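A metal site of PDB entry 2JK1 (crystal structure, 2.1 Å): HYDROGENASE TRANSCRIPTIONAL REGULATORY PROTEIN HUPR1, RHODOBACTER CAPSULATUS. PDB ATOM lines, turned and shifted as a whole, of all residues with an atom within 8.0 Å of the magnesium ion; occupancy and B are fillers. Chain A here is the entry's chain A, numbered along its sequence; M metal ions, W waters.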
ATOM      1  N   VAL A   7      -3.832 -33.581  11.803  1.00  0.00           N
ATOM      2  CA  VAL A   7      -3.298 -33.060  10.545  1.00  0.00           C
ATOM      3  C   VAL A   7      -4.142 -31.860  10.108  1.00  0.00           C
ATOM      4  O   VAL A   7      -5.334 -31.994   9.870  1.00  0.00           O
ATOM      5  CB  VAL A   7      -3.324 -34.110   9.397  1.00  0.00           C
ATOM      6  CG1 VAL A   7      -2.527 -33.602   8.192  1.00  0.00           C
ATOM      7  CG2 VAL A   7      -2.823 -35.493   9.859  1.00  0.00           C
ATOM      8  N   ASP A   8      -3.498 -30.689  10.047  1.00  0.00           N
ATOM      9  CA  ASP A   8      -4.164 -29.436   9.718  1.00  0.00           C
ATOM     10  C   ASP A   8      -3.090 -28.472   9.211  1.00  0.00           C
ATOM     11  O   ASP A   8      -2.019 -28.375   9.795  1.00  0.00           O
ATOM     12  CB  ASP A   8      -4.827 -28.857  10.964  1.00  0.00           C
ATOM     13  CG  ASP A   8      -5.893 -27.818  10.649  1.00  0.00           C
ATOM     14  OD1 ASP A   8      -5.816 -27.164   9.591  1.00  0.00           O
ATOM     15  OD2 ASP A   8      -6.856 -27.674  11.448  1.00  0.00           O
ATOM     16  N   ASP A   9      -3.406 -27.744   8.138  1.00  0.00           N
ATOM     17  CA  ASP A   9      -2.428 -26.866   7.503  1.00  0.00           C
ATOM     18  C   ASP A   9      -2.276 -25.551   8.260  1.00  0.00           C
ATOM     19  O   ASP A   9      -1.223 -24.922   8.187  1.00  0.00           O
ATOM     20  CB  ASP A   9      -2.734 -26.649   6.007  1.00  0.00           C
ATOM     21  CG  ASP A   9      -4.141 -26.120   5.738  1.00  0.00           C
ATOM     22  OD1 ASP A   9      -5.141 -26.732   6.199  1.00  0.00           O
ATOM     23  OD2 ASP A   9      -4.258 -25.088   5.046  1.00  0.00           O
ATOM     24  N   GLU A  10      -3.316 -25.159   9.016  1.00  0.00           N
ATOM     25  CA  GLU A  10      -3.314 -23.904   9.765  1.00  0.00           C
ATOM     26  C   GLU A  10      -2.762 -24.103  11.179  1.00  0.00           C
ATOM     27  O   GLU A  10      -3.354 -24.822  11.968  1.00  0.00           O
ATOM     28  CB  GLU A  10      -4.729 -23.298   9.788  1.00  0.00           C
ATOM     29  CG  GLU A  10      -5.520 -23.579   8.510  1.00  0.00           C
ATOM     30  CD  GLU A  10      -6.628 -22.592   8.223  1.00  0.00           C
ATOM     31  OE1 GLU A  10      -7.507 -22.385   9.113  1.00  0.00           O
ATOM     32  OE2 GLU A  10      -6.659 -22.045   7.082  1.00  0.00           O
ATOM     33  N   SER A  13      -5.030 -23.649  14.559  1.00  0.00           N
ATOM     34  CA  SER A  13      -6.058 -24.679  14.693  1.00  0.00           C
ATOM     35  C   SER A  13      -5.383 -25.958  15.156  1.00  0.00           C
ATOM     36  O   SER A  13      -5.884 -26.638  16.053  1.00  0.00           O
ATOM     37  CB  SER A  13      -6.815 -24.925  13.392  1.00  0.00           C
ATOM     38  OG  SER A  13      -7.587 -26.124  13.503  1.00  0.00           O
ATOM     39  N   GLN A  31       1.512 -30.934   9.442  1.00  0.00           N
ATOM     40  CA  GLN A  31       0.958 -29.767   8.755  1.00  0.00           C
ATOM     41  C   GLN A  31       0.328 -30.058   7.369  1.00  0.00           C
ATOM     42  O   GLN A  31      -0.238 -29.169   6.750  1.00  0.00           O
ATOM     43  CB  GLN A  31       2.022 -28.667   8.608  1.00  0.00           C
ATOM     44  CG  GLN A  31       2.339 -27.914   9.895  1.00  0.00           C
ATOM     45  CD  GLN A  31       3.048 -26.587   9.607  1.00  0.00           C
ATOM     46  OE1 GLN A  31       4.248 -26.547   9.266  1.00  0.00           O
ATOM     47  NE2 GLN A  31       2.301 -25.486   9.741  1.00  0.00           N
ATOM     48  N   CYS A  50      -8.103 -35.308  10.564  1.00  0.00           N
ATOM     49  CA  CYS A  50      -7.541 -34.595   9.450  1.00  0.00           C
ATOM     50  C   CYS A  50      -8.460 -33.534   8.839  1.00  0.00           C
ATOM     51  O   CYS A  50      -9.652 -33.773   8.585  1.00  0.00           O
ATOM     52  CB  CYS A  50      -7.106 -35.626   8.397  1.00  0.00           C
ATOM     53  SG  CYS A  50      -6.226 -34.902   7.046  1.00  0.00           S
ATOM     54  N   ASP A  51      -7.928 -32.335   8.608  1.00  0.00           N
ATOM     55  CA  ASP A  51      -8.658 -31.291   7.936  1.00  0.00           C
ATOM     56  C   ASP A  51      -8.805 -31.633   6.438  1.00  0.00           C
ATOM     57  O   ASP A  51      -7.889 -32.216   5.856  1.00  0.00           O
ATOM     58  CB  ASP A  51      -7.891 -29.979   8.130  1.00  0.00           C
ATOM     59  CG  ASP A  51      -8.563 -28.797   7.442  1.00  0.00           C
ATOM     60  OD1 ASP A  51      -9.727 -28.475   7.687  1.00  0.00           O
ATOM     61  OD2 ASP A  51      -7.898 -28.196   6.642  1.00  0.00           O
ATOM     62  N   GLN A  52      -9.954 -31.331   5.825  1.00  0.00           N
ATOM     63  CA  GLN A  52     -10.161 -31.626   4.421  1.00  0.00           C
ATOM     64  C   GLN A  52      -9.313 -30.733   3.491  1.00  0.00           C
ATOM     65  O   GLN A  52      -8.617 -31.232   2.605  1.00  0.00           O
ATOM     66  CB  GLN A  52     -11.645 -31.543   4.042  1.00  0.00           C
ATOM     67  CG  GLN A  52     -11.969 -31.444   2.532  1.00  0.00           C
ATOM     68  CD  GLN A  52     -11.462 -32.640   1.729  1.00  0.00           C
ATOM     69  OE1 GLN A  52     -10.903 -33.583   2.278  1.00  0.00           O
ATOM     70  NE2 GLN A  52     -11.650 -32.577   0.415  1.00  0.00           N
ATOM     71  N   ARG A  53      -9.372 -29.425   3.708  1.00  0.00           N
ATOM     72  CA  ARG A  53      -8.826 -28.475   2.729  1.00  0.00           C
ATOM     73  C   ARG A  53      -7.416 -28.079   3.164  1.00  0.00           C
ATOM     74  O   ARG A  53      -7.260 -27.322   4.123  1.00  0.00           O
ATOM     75  CB  ARG A  53      -9.767 -27.260   2.556  1.00  0.00           C
ATOM     76  CG  ARG A  53     -11.034 -27.540   1.707  1.00  0.00           C
ATOM     77  CD  ARG A  53     -11.889 -26.272   1.429  1.00  0.00           C
ATOM     78  NE  ARG A  53     -12.585 -25.830   2.641  1.00  0.00           N
ATOM     79  CZ  ARG A  53     -13.319 -24.725   2.776  1.00  0.00           C
ATOM     80  NH1 ARG A  53     -13.468 -23.881   1.751  1.00  0.00           N
ATOM     81  NH2 ARG A  53     -13.888 -24.466   3.959  1.00  0.00           N
ATOM     82  N   MET A  54      -6.420 -28.660   2.500  1.00  0.00           N
ATOM     83  CA  MET A  54      -5.008 -28.409   2.753  1.00  0.00           C
ATOM     84  C   MET A  54      -4.281 -28.186   1.400  1.00  0.00           C
ATOM     85  O   MET A  54      -4.638 -28.835   0.405  1.00  0.00           O
ATOM     86  CB  MET A  54      -4.352 -29.597   3.491  1.00  0.00           C
ATOM     87  CG  MET A  54      -5.042 -29.988   4.840  1.00  0.00           C
ATOM     88  SD  MET A  54      -4.096 -31.218   5.736  1.00  0.00           S
ATOM     89  CE  MET A  54      -4.357 -32.692   4.722  1.00  0.00           C
ATOM     90  N   PRO A  55      -3.259 -27.307   1.365  1.00  0.00           N
ATOM     91  CA  PRO A  55      -2.587 -27.068   0.072  1.00  0.00           C
ATOM     92  C   PRO A  55      -2.089 -28.383  -0.525  1.00  0.00           C
ATOM     93  O   PRO A  55      -1.495 -29.215   0.178  1.00  0.00           O
ATOM     94  CB  PRO A  55      -1.440 -26.118   0.423  1.00  0.00           C
ATOM     95  CG  PRO A  55      -1.789 -25.507   1.739  1.00  0.00           C
ATOM     96  CD  PRO A  55      -2.635 -26.539   2.464  1.00  0.00           C
ATOM     97  N   ILE A  78     -12.307 -33.339   9.256  1.00  0.00           N
ATOM     98  CA  ILE A  78     -12.930 -32.073   9.596  1.00  0.00           C
ATOM     99  C   ILE A  78     -13.195 -31.343   8.291  1.00  0.00           C
ATOM    100  O   ILE A  78     -12.290 -31.172   7.498  1.00  0.00           O
ATOM    101  CB  ILE A  78     -12.014 -31.211  10.528  1.00  0.00           C
ATOM    102  CG1 ILE A  78     -11.769 -31.995  11.854  1.00  0.00           C
ATOM    103  CG2 ILE A  78     -12.671 -29.814  10.800  1.00  0.00           C
ATOM    104  CD1 ILE A  78     -10.583 -31.453  12.657  1.00  0.00           C
ATOM    105  N   LYS A 102     -16.796 -28.081  10.270  1.00  0.00           N
ATOM    106  CA  LYS A 102     -15.898 -26.928  10.460  1.00  0.00           C
ATOM    107  C   LYS A 102     -16.708 -25.644  10.810  1.00  0.00           C
ATOM    108  O   LYS A 102     -17.777 -25.445  10.225  1.00  0.00           O
ATOM    109  CB  LYS A 102     -15.113 -26.750   9.148  1.00  0.00           C
ATOM    110  CG  LYS A 102     -13.684 -26.307   9.251  1.00  0.00           C
ATOM    111  CD  LYS A 102     -12.925 -26.636   7.958  1.00  0.00           C
ATOM    112  CE  LYS A 102     -11.798 -25.648   7.682  1.00  0.00           C
ATOM    113  NZ  LYS A 102     -10.772 -25.501   8.819  1.00  0.00           N
HETATM  114 MG    MG M   1      -7.109 -26.355   6.019  1.00  0.00          MG
HETATM  115  O   HOH W   1      -7.378 -25.831   8.118  1.00  0.00           O
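OD1 of Asp 8 is in hydrogen-bond range of N of Glu 10, 3.3 Å away.
OD2 of Asp 8 lies within hydrogen-bond range of OG of Ser 13 (2.7 Å).
OD1 of Asp 51 lies within salt-bridge range of NZ of Lys 102, 3.3 Å away.
The backbone NH (N) of Asp 51 is in hydrogen-bond range of the backbone carbonyl oxygen (O) of Val 7 (2.9 Å).
Merely in contact with the magnesium ion: Asp 8 (3.9 Å).
Within 4 Å of the magnesium ion: Asp 8, Asp 9, Asp 51 and Arg 53.
The magnesium ion is bound by the side-chain carboxylate (OD1) of Asp 9 (2.0 Å), the side-chain carboxylate (OD2) of Asp 51 (2.1 Å), the backbone carbonyl oxygen (O) of Arg 53 (2.1 Å) and water W1 (2.2 Å).
Water W1 lies within hydrogen-bond range of OD1 of Asp 8 and NZ of Lys 102.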
